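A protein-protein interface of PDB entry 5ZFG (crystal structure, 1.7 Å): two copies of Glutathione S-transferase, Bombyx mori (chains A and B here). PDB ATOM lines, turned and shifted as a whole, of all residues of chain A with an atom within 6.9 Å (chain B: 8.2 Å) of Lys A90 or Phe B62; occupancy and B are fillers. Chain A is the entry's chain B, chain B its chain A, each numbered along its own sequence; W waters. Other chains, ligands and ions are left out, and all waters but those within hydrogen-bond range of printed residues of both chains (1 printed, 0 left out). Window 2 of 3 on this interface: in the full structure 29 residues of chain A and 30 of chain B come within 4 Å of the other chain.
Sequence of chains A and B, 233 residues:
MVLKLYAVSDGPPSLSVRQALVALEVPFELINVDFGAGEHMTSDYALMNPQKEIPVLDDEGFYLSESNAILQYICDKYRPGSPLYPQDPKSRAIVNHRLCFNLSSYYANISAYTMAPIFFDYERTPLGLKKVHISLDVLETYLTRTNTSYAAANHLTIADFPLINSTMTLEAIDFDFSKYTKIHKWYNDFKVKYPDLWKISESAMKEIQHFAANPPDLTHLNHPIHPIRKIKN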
ATOM      1  N   GLN A  87       9.181  20.896  20.137  1.00  0.00           N
ATOM      2  CA  GLN A  87       8.555  19.623  19.812  1.00  0.00           C
ATOM      3  C   GLN A  87       9.428  18.428  20.159  1.00  0.00           C
ATOM      4  O   GLN A  87       8.905  17.319  20.280  1.00  0.00           O
ATOM      5  CB  GLN A  87       8.189  19.579  18.323  1.00  0.00           C
ATOM      6  CG  GLN A  87       7.201  20.660  17.925  1.00  0.00           C
ATOM      7  CD  GLN A  87       6.972  20.724  16.428  1.00  0.00           C
ATOM      8  OE1 GLN A  87       5.914  20.323  15.935  1.00  0.00           O
ATOM      9  NE2 GLN A  87       7.959  21.239  15.695  1.00  0.00           N
ATOM     10  N   ASP A  88      10.732  18.626  20.324  1.00  0.00           N
ATOM     11  CA  ASP A  88      11.604  17.529  20.710  1.00  0.00           C
ATOM     12  C   ASP A  88      11.136  16.977  22.054  1.00  0.00           C
ATOM     13  O   ASP A  88      10.985  17.751  23.008  1.00  0.00           O
ATOM     14  CB  ASP A  88      13.044  18.001  20.825  1.00  0.00           C
ATOM     15  CG  ASP A  88      13.936  16.959  21.461  1.00  0.00           C
ATOM     16  OD1 ASP A  88      14.151  15.900  20.817  1.00  0.00           O
ATOM     17  OD2 ASP A  88      14.403  17.185  22.605  1.00  0.00           O
ATOM     18  N   PRO A  89      10.926  15.664  22.180  1.00  0.00           N
ATOM     19  CA  PRO A  89      10.319  15.138  23.421  1.00  0.00           C
ATOM     20  C   PRO A  89      11.064  15.511  24.691  1.00  0.00           C
ATOM     21  O   PRO A  89      10.421  15.901  25.674  1.00  0.00           O
ATOM     22  CB  PRO A  89      10.305  13.622  23.170  1.00  0.00           C
ATOM     23  CG  PRO A  89      10.158  13.524  21.665  1.00  0.00           C
ATOM     24  CD  PRO A  89      11.042  14.625  21.144  1.00  0.00           C
ATOM     25  N   LYS A  90      12.396  15.387  24.716  1.00  0.00           N
ATOM     26  CA  LYS A  90      13.147  15.744  25.918  1.00  0.00           C
ATOM     27  C   LYS A  90      13.046  17.235  26.220  1.00  0.00           C
ATOM     28  O   LYS A  90      12.803  17.632  27.367  1.00  0.00           O
ATOM     29  CB  LYS A  90      14.612  15.329  25.775  1.00  0.00           C
ATOM     30  CG  LYS A  90      15.442  15.608  27.017  1.00  0.00           C
ATOM     31  CD  LYS A  90      16.849  15.055  26.867  1.00  0.00           C
ATOM     32  CE  LYS A  90      17.772  15.618  27.931  1.00  0.00           C
ATOM     33  NZ  LYS A  90      19.139  15.042  27.771  1.00  0.00           N
ATOM     34  N   SER A  91      13.251  18.082  25.206  1.00  0.00           N
ATOM     35  CA  SER A  91      13.153  19.522  25.436  1.00  0.00           C
ATOM     36  C   SER A  91      11.738  19.907  25.857  1.00  0.00           C
ATOM     37  O   SER A  91      11.547  20.781  26.716  1.00  0.00           O
ATOM     38  CB  SER A  91      13.568  20.286  24.177  1.00  0.00           C
ATOM     39  OG  SER A  91      14.784  19.768  23.651  1.00  0.00           O
ATOM     40  N   ARG A  92      10.741  19.249  25.270  1.00  0.00           N
ATOM     41  CA  ARG A  92       9.357  19.522  25.643  1.00  0.00           C
ATOM     42  C   ARG A  92       9.073  19.079  27.073  1.00  0.00           C
ATOM     43  O   ARG A  92       8.330  19.754  27.804  1.00  0.00           O
ATOM     44  CB  ARG A  92       8.405  18.833  24.667  1.00  0.00           C
ATOM     45  CG  ARG A  92       6.932  18.957  25.050  1.00  0.00           C
ATOM     46  CD  ARG A  92       6.032  18.781  23.833  1.00  0.00           C
ATOM     47  NE  ARG A  92       6.160  19.896  22.898  1.00  0.00           N
ATOM     48  CZ  ARG A  92       5.162  20.381  22.171  1.00  0.00           C
ATOM     49  NH1 ARG A  92       5.376  21.400  21.351  1.00  0.00           N
ATOM     50  NH2 ARG A  92       3.951  19.854  22.262  1.00  0.00           N
ATOM     51  N   ALA A  93       9.667  17.957  27.494  1.00  0.00           N
ATOM     52  CA  ALA A  93       9.480  17.476  28.864  1.00  0.00           C
ATOM     53  C   ALA A  93      10.017  18.463  29.892  1.00  0.00           C
ATOM     54  O   ALA A  93       9.432  18.617  30.973  1.00  0.00           O
ATOM     55  CB  ALA A  93      10.146  16.123  29.036  1.00  0.00           C
ATOM     56  N   ILE A  94      11.144  19.119  29.595  1.00  0.00           N
ATOM     57  CA  ILE A  94      11.668  20.116  30.531  1.00  0.00           C
ATOM     58  C   ILE A  94      10.672  21.263  30.687  1.00  0.00           C
ATOM     59  O   ILE A  94      10.406  21.724  31.807  1.00  0.00           O
ATOM     60  CB  ILE A  94      13.057  20.623  30.090  1.00  0.00           C
ATOM     61  CG1 ILE A  94      14.056  19.453  29.973  1.00  0.00           C
ATOM     62  CG2 ILE A  94      13.597  21.653  31.111  1.00  0.00           C
ATOM     63  CD1 ILE A  94      15.347  19.822  29.243  1.00  0.00           C
ATOM     64  N   VAL A  95      10.092  21.726  29.572  1.00  0.00           N
ATOM     65  CA  VAL A  95       9.048  22.748  29.646  1.00  0.00           C
ATOM     66  C   VAL A  95       7.862  22.246  30.460  1.00  0.00           C
ATOM     67  O   VAL A  95       7.388  22.935  31.375  1.00  0.00           O
ATOM     68  CB  VAL A  95       8.605  23.192  28.239  1.00  0.00           C
ATOM     69  CG1 VAL A  95       7.385  24.148  28.346  1.00  0.00           C
ATOM     70  CG2 VAL A  95       9.768  23.874  27.511  1.00  0.00           C
ATOM     71  N   ALA A 152      13.762  26.606  30.933  1.00  0.00           N
ATOM     72  CA  ALA A 152      13.766  25.278  30.329  1.00  0.00           C
ATOM     73  C   ALA A 152      14.751  25.132  29.179  1.00  0.00           C
ATOM     74  O   ALA A 152      14.883  24.032  28.630  1.00  0.00           O
ATOM     75  CB  ALA A 152      12.356  24.906  29.836  1.00  0.00           C
ATOM     76  N   LEU B   3      14.274   2.038  31.140  1.00  0.00           N
ATOM     77  CA  LEU B   3      13.899   3.167  31.981  1.00  0.00           C
ATOM     78  C   LEU B   3      13.982   2.744  33.443  1.00  0.00           C
ATOM     79  O   LEU B   3      13.768   1.579  33.778  1.00  0.00           O
ATOM     80  CB  LEU B   3      12.473   3.629  31.665  1.00  0.00           C
ATOM     81  CG  LEU B   3      12.203   4.641  30.558  1.00  0.00           C
ATOM     82  CD1 LEU B   3      12.688   4.109  29.232  1.00  0.00           C
ATOM     83  CD2 LEU B   3      10.724   4.934  30.481  1.00  0.00           C
ATOM     84  N   LYS B   4      14.268   3.699  34.325  1.00  0.00           N
ATOM     85  CA  LYS B   4      14.238   3.455  35.764  1.00  0.00           C
ATOM     86  C   LYS B   4      13.195   4.379  36.377  1.00  0.00           C
ATOM     87  O   LYS B   4      13.258   5.597  36.174  1.00  0.00           O
ATOM     88  CB  LYS B   4      15.606   3.691  36.398  1.00  0.00           C
ATOM     89  CG  LYS B   4      16.645   2.624  35.995  1.00  0.00           C
ATOM     90  CD  LYS B   4      18.057   3.044  36.364  1.00  0.00           C
ATOM     91  CE  LYS B   4      18.571   2.259  37.551  1.00  0.00           C
ATOM     92  NZ  LYS B   4      20.056   2.173  37.531  1.00  0.00           N
ATOM     93  N   MET B  48      18.440  13.379  41.566  1.00  0.00           N
ATOM     94  CA  MET B  48      17.452  13.089  40.534  1.00  0.00           C
ATOM     95  C   MET B  48      16.265  14.041  40.603  1.00  0.00           C
ATOM     96  O   MET B  48      15.808  14.538  39.568  1.00  0.00           O
ATOM     97  CB  MET B  48      16.968  11.643  40.661  1.00  0.00           C
ATOM     98  CG  MET B  48      18.022  10.581  40.394  1.00  0.00           C
ATOM     99  SD  MET B  48      17.317   8.911  40.411  1.00  0.00           S
ATOM    100  CE  MET B  48      16.781   8.773  42.123  1.00  0.00           C
ATOM    101  N   VAL B  56      10.069   9.758  40.399  1.00  0.00           N
ATOM    102  CA  VAL B  56      11.022  10.393  39.493  1.00  0.00           C
ATOM    103  C   VAL B  56      11.489   9.340  38.500  1.00  0.00           C
ATOM    104  O   VAL B  56      11.697   8.179  38.867  1.00  0.00           O
ATOM    105  CB  VAL B  56      12.211  11.046  40.242  1.00  0.00           C
ATOM    106  CG1 VAL B  56      13.055  10.028  41.014  1.00  0.00           C
ATOM    107  CG2 VAL B  56      13.084  11.848  39.277  1.00  0.00           C
ATOM    108  N   LEU B  57      11.624   9.748  37.240  1.00  0.00           N
ATOM    109  CA  LEU B  57      12.068   8.883  36.149  1.00  0.00           C
ATOM    110  C   LEU B  57      13.537   9.138  35.843  1.00  0.00           C
ATOM    111  O   LEU B  57      13.990  10.285  35.840  1.00  0.00           O
ATOM    112  CB  LEU B  57      11.220   9.138  34.898  1.00  0.00           C
ATOM    113  CG  LEU B  57      11.461   8.204  33.712  1.00  0.00           C
ATOM    114  CD1 LEU B  57      10.819   6.844  33.948  1.00  0.00           C
ATOM    115  CD2 LEU B  57      10.960   8.828  32.389  1.00  0.00           C
ATOM    116  N   ASP B  58      14.288   8.062  35.601  1.00  0.00           N
ATOM    117  CA  ASP B  58      15.653   8.154  35.081  1.00  0.00           C
ATOM    118  C   ASP B  58      15.688   7.429  33.737  1.00  0.00           C
ATOM    119  O   ASP B  58      15.657   6.194  33.689  1.00  0.00           O
ATOM    120  CB  ASP B  58      16.658   7.567  36.079  1.00  0.00           C
ATOM    121  CG  ASP B  58      18.067   7.408  35.491  1.00  0.00           C
ATOM    122  OD1 ASP B  58      18.337   7.901  34.373  1.00  0.00           O
ATOM    123  OD2 ASP B  58      18.913   6.783  36.167  1.00  0.00           O
ATOM    124  N   ASP B  59      15.740   8.199  32.648  1.00  0.00           N
ATOM    125  CA  ASP B  59      15.774   7.657  31.283  1.00  0.00           C
ATOM    126  C   ASP B  59      17.197   7.871  30.783  1.00  0.00           C
ATOM    127  O   ASP B  59      17.522   8.911  30.207  1.00  0.00           O
ATOM    128  CB  ASP B  59      14.743   8.327  30.363  1.00  0.00           C
ATOM    129  CG  ASP B  59      14.525   7.559  29.066  1.00  0.00           C
ATOM    130  OD1 ASP B  59      15.076   6.435  28.926  1.00  0.00           O
ATOM    131  OD2 ASP B  59      13.789   8.065  28.184  1.00  0.00           O
ATOM    132  N   GLU B  60      18.048   6.881  31.049  1.00  0.00           N
ATOM    133  CA  GLU B  60      19.449   6.885  30.631  1.00  0.00           C
ATOM    134  C   GLU B  60      20.130   8.210  30.971  1.00  0.00           C
ATOM    135  O   GLU B  60      20.834   8.804  30.156  1.00  0.00           O
ATOM    136  CB  GLU B  60      19.561   6.549  29.141  1.00  0.00           C
ATOM    137  CG  GLU B  60      18.939   5.181  28.796  1.00  0.00           C
ATOM    138  CD  GLU B  60      19.083   4.791  27.331  1.00  0.00           C
ATOM    139  OE1 GLU B  60      18.166   4.129  26.793  1.00  0.00           O
ATOM    140  OE2 GLU B  60      20.114   5.139  26.719  1.00  0.00           O
ATOM    141  N   GLY B  61      19.900   8.684  32.205  1.00  0.00           N
ATOM    142  CA  GLY B  61      20.548   9.867  32.728  1.00  0.00           C
ATOM    143  C   GLY B  61      19.714  11.132  32.672  1.00  0.00           C
ATOM    144  O   GLY B  61      20.092  12.133  33.290  1.00  0.00           O
ATOM    145  N   PHE B  62      18.602  11.115  31.948  1.00  0.00           N
ATOM    146  CA  PHE B  62      17.648  12.219  31.953  1.00  0.00           C
ATOM    147  C   PHE B  62      16.712  12.018  33.139  1.00  0.00           C
ATOM    148  O   PHE B  62      15.936  11.059  33.153  1.00  0.00           O
ATOM    149  CB  PHE B  62      16.876  12.251  30.638  1.00  0.00           C
ATOM    150  CG  PHE B  62      15.804  13.304  30.579  1.00  0.00           C
ATOM    151  CD1 PHE B  62      16.101  14.625  30.859  1.00  0.00           C
ATOM    152  CD2 PHE B  62      14.509  12.974  30.206  1.00  0.00           C
ATOM    153  CE1 PHE B  62      15.114  15.605  30.791  1.00  0.00           C
ATOM    154  CE2 PHE B  62      13.523  13.952  30.135  1.00  0.00           C
ATOM    155  CZ  PHE B  62      13.836  15.261  30.426  1.00  0.00           C
ATOM    156  N   TYR B  63      16.801  12.898  34.133  1.00  0.00           N
ATOM    157  CA  TYR B  63      15.981  12.829  35.343  1.00  0.00           C
ATOM    158  C   TYR B  63      14.761  13.728  35.202  1.00  0.00           C
ATOM    159  O   TYR B  63      14.899  14.945  35.069  1.00  0.00           O
ATOM    160  CB  TYR B  63      16.775  13.257  36.576  1.00  0.00           C
ATOM    161  CG  TYR B  63      18.033  12.454  36.800  1.00  0.00           C
ATOM    162  CD1 TYR B  63      18.045  11.081  36.596  1.00  0.00           C
ATOM    163  CD2 TYR B  63      19.208  13.072  37.203  1.00  0.00           C
ATOM    164  CE1 TYR B  63      19.193  10.334  36.797  1.00  0.00           C
ATOM    165  CE2 TYR B  63      20.359  12.339  37.406  1.00  0.00           C
ATOM    166  CZ  TYR B  63      20.346  10.972  37.199  1.00  0.00           C
ATOM    167  OH  TYR B  63      21.488  10.230  37.402  1.00  0.00           O
ATOM    168  N   LEU B  64      13.570  13.142  35.290  1.00  0.00           N
ATOM    169  CA  LEU B  64      12.333  13.893  35.109  1.00  0.00           C
ATOM    170  C   LEU B  64      11.385  13.571  36.258  1.00  0.00           C
ATOM    171  O   LEU B  64      10.976  12.419  36.419  1.00  0.00           O
ATOM    172  CB  LEU B  64      11.706  13.552  33.748  1.00  0.00           C
ATOM    173  CG  LEU B  64      10.378  14.242  33.444  1.00  0.00           C
ATOM    174  CD1 LEU B  64      10.623  15.736  33.245  1.00  0.00           C
ATOM    175  CD2 LEU B  64       9.729  13.631  32.218  1.00  0.00           C
ATOM    176  N   SER B  65      11.036  14.583  37.062  1.00  0.00           N
ATOM    177  CA  SER B  65       9.995  14.421  38.069  1.00  0.00           C
ATOM    178  C   SER B  65       8.697  15.057  37.568  1.00  0.00           C
ATOM    179  O   SER B  65       8.616  15.490  36.408  1.00  0.00           O
ATOM    180  CB  SER B  65      10.426  15.032  39.405  1.00  0.00           C
ATOM    181  OG  SER B  65      10.514  16.446  39.329  1.00  0.00           O
ATOM    182  N   ALA B  69       4.166  15.400  33.898  1.00  0.00           N
ATOM    183  CA  ALA B  69       5.195  15.591  32.877  1.00  0.00           C
ATOM    184  C   ALA B  69       5.807  14.260  32.454  1.00  0.00           C
ATOM    185  O   ALA B  69       6.128  14.064  31.275  1.00  0.00           O
ATOM    186  CB  ALA B  69       6.281  16.528  33.402  1.00  0.00           C
ATOM    187  N   ILE B  70       5.962  13.333  33.405  1.00  0.00           N
ATOM    188  CA  ILE B  70       6.475  12.004  33.064  1.00  0.00           C
ATOM    189  C   ILE B  70       5.513  11.295  32.120  1.00  0.00           C
ATOM    190  O   ILE B  70       5.928  10.701  31.115  1.00  0.00           O
ATOM    191  CB  ILE B  70       6.718  11.166  34.333  1.00  0.00           C
ATOM    192  CG1 ILE B  70       7.833  11.783  35.182  1.00  0.00           C
ATOM    193  CG2 ILE B  70       7.056   9.710  33.912  1.00  0.00           C
ATOM    194  CD1 ILE B  70       7.922  11.189  36.604  1.00  0.00           C
ATOM    195  N   TYR B  73       5.873  12.730  28.709  1.00  0.00           N
ATOM    196  CA  TYR B  73       7.166  12.440  28.093  1.00  0.00           C
ATOM    197  C   TYR B  73       7.210  11.023  27.542  1.00  0.00           C
ATOM    198  O   TYR B  73       7.666  10.799  26.417  1.00  0.00           O
ATOM    199  CB  TYR B  73       8.281  12.654  29.112  1.00  0.00           C
ATOM    200  CG  TYR B  73       9.631  12.081  28.694  1.00  0.00           C
ATOM    201  CD1 TYR B  73      10.359  12.665  27.670  1.00  0.00           C
ATOM    202  CD2 TYR B  73      10.147  10.951  29.312  1.00  0.00           C
ATOM    203  CE1 TYR B  73      11.585  12.156  27.276  1.00  0.00           C
ATOM    204  CE2 TYR B  73      11.377  10.419  28.921  1.00  0.00           C
ATOM    205  CZ  TYR B  73      12.086  11.035  27.907  1.00  0.00           C
ATOM    206  OH  TYR B  73      13.314  10.541  27.516  1.00  0.00           O
ATOM    207  N   ILE B  74       6.734  10.047  28.317  1.00  0.00           N
ATOM    208  CA  ILE B  74       6.845   8.687  27.817  1.00  0.00           C
ATOM    209  C   ILE B  74       5.999   8.507  26.559  1.00  0.00           C
ATOM    210  O   ILE B  74       6.412   7.781  25.643  1.00  0.00           O
ATOM    211  CB  ILE B  74       6.513   7.663  28.920  1.00  0.00           C
ATOM    212  CG1 ILE B  74       5.128   7.887  29.491  1.00  0.00           C
ATOM    213  CG2 ILE B  74       7.553   7.732  30.036  1.00  0.00           C
ATOM    214  CD1 ILE B  74       4.835   6.996  30.704  1.00  0.00           C
ATOM    215  N   ASP B  76       5.268  11.131  24.334  1.00  0.00           N
ATOM    216  CA  ASP B  76       5.953  11.925  23.306  1.00  0.00           C
ATOM    217  C   ASP B  76       7.205  11.222  22.790  1.00  0.00           C
ATOM    218  O   ASP B  76       7.478  11.234  21.583  1.00  0.00           O
ATOM    219  CB  ASP B  76       6.352  13.298  23.853  1.00  0.00           C
ATOM    220  CG  ASP B  76       5.154  14.217  24.130  1.00  0.00           C
ATOM    221  OD1 ASP B  76       4.041  13.956  23.615  1.00  0.00           O
ATOM    222  OD2 ASP B  76       5.357  15.212  24.873  1.00  0.00           O
ATOM    223  N   LYS B  77       7.991  10.625  23.687  1.00  0.00           N
ATOM    224  CA  LYS B  77       9.266  10.027  23.303  1.00  0.00           C
ATOM    225  C   LYS B  77       9.079   8.650  22.671  1.00  0.00           C
ATOM    226  O   LYS B  77       9.656   8.351  21.620  1.00  0.00           O
ATOM    227  CB  LYS B  77      10.177   9.940  24.533  1.00  0.00           C
ATOM    228  CG  LYS B  77      11.486   9.207  24.297  1.00  0.00           C
ATOM    229  CD  LYS B  77      12.427  10.024  23.435  1.00  0.00           C
ATOM    230  CE  LYS B  77      13.732   9.268  23.183  1.00  0.00           C
ATOM    231  NZ  LYS B  77      14.560   9.912  22.119  1.00  0.00           N
ATOM    232  N   TYR B  78       8.279   7.789  23.302  1.00  0.00           N
ATOM    233  CA  TYR B  78       8.256   6.392  22.866  1.00  0.00           C
ATOM    234  C   TYR B  78       7.035   5.974  22.067  1.00  0.00           C
ATOM    235  O   TYR B  78       7.116   4.978  21.341  1.00  0.00           O
ATOM    236  CB  TYR B  78       8.417   5.461  24.073  1.00  0.00           C
ATOM    237  CG  TYR B  78       9.774   5.665  24.657  1.00  0.00           C
ATOM    238  CD1 TYR B  78      10.921   5.354  23.914  1.00  0.00           C
ATOM    239  CD2 TYR B  78       9.932   6.233  25.906  1.00  0.00           C
ATOM    240  CE1 TYR B  78      12.176   5.583  24.427  1.00  0.00           C
ATOM    241  CE2 TYR B  78      11.177   6.460  26.425  1.00  0.00           C
ATOM    242  CZ  TYR B  78      12.299   6.129  25.686  1.00  0.00           C
ATOM    243  OH  TYR B  78      13.544   6.366  26.205  1.00  0.00           O
HETATM  244  O   HOH W   1       7.625  15.344  26.539  1.00  0.00           O
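Pro A89 touches Tyr B73 (O to CD1, 3.8 Å).
Asp B76 touches Pro A89.
Lys B77 touches Pro A89 (CA to CB, 3.7 Å).
CE of Lys A90 touches CD1 of Phe B62, at 3.5 Å.
Asp B76 touches Arg A92.
Leu B64 touches Ala A93 (CD1 to O, 3.9 Å).
Ala A93 touches Tyr B73.
Of the 10 printed residues of chain A, 4 touch a printed residue of chain B.
Printed residues of chain A that touch a printed residue of chain B: Pro A89, Lys A90, Arg A92 and Ala A93.
Hydrophobic or aromatic side chains of chain A that line the printed part of chain B: Pro A89 and Ala A93.
Hydrophobic or aromatic side chains of chain B that line the printed part of chain A: Phe B62, Leu B64 and Tyr B73.
Among the printed residues, no Asp or Glu carboxylate lies within 4 Å of a Lys or Arg side-chain nitrogen of the other chain.
The side-chain carboxylate of Asp A88 sits close to the backbone NH of Lys A90, 3.4 Å away.
OD2 of Asp B59 is in hydrogen-bond range of OH of Tyr B73 (2.6 Å).
N of Leu B57 is in hydrogen-bond range of O of Leu B64, at 2.9 Å.
Of chain B, only Phe B62 (3.5 Å) comes within 4 Å of Lys A90.
No residue of chain B comes within 4 Å of Ser A91.
Printed residues of chain B within 4 Å of Arg A92: Asp B76 (3.8 Å).
No residue of chain A comes within 4 Å of Gly B61.
Phe B62 touches one residue of chain A.
Printed residues of chain A within 4 Å of Leu B64: Ala A93 (3.9 Å).
Printed residues of chain A within 4 Å of Asp B76: Pro A89 (3.5 Å) and Arg A92 (3.8 Å).
Of the printed residues of chain A, Lys B77 touches Pro A89.
The nearest residue of chain A that does not touch Phe B62 is Ala A93 (4.04 Å).
Water W1 lies within hydrogen-bond range of the side-chain carboxylate of Asp B76, the backbone carbonyl oxygen of Pro A89 and the backbone NH of Ala A93.
No position is printed for both chains.
Of the 7 pairs that touch across the chains among the printed residues, none has its exchanged pair printed and touching as well.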
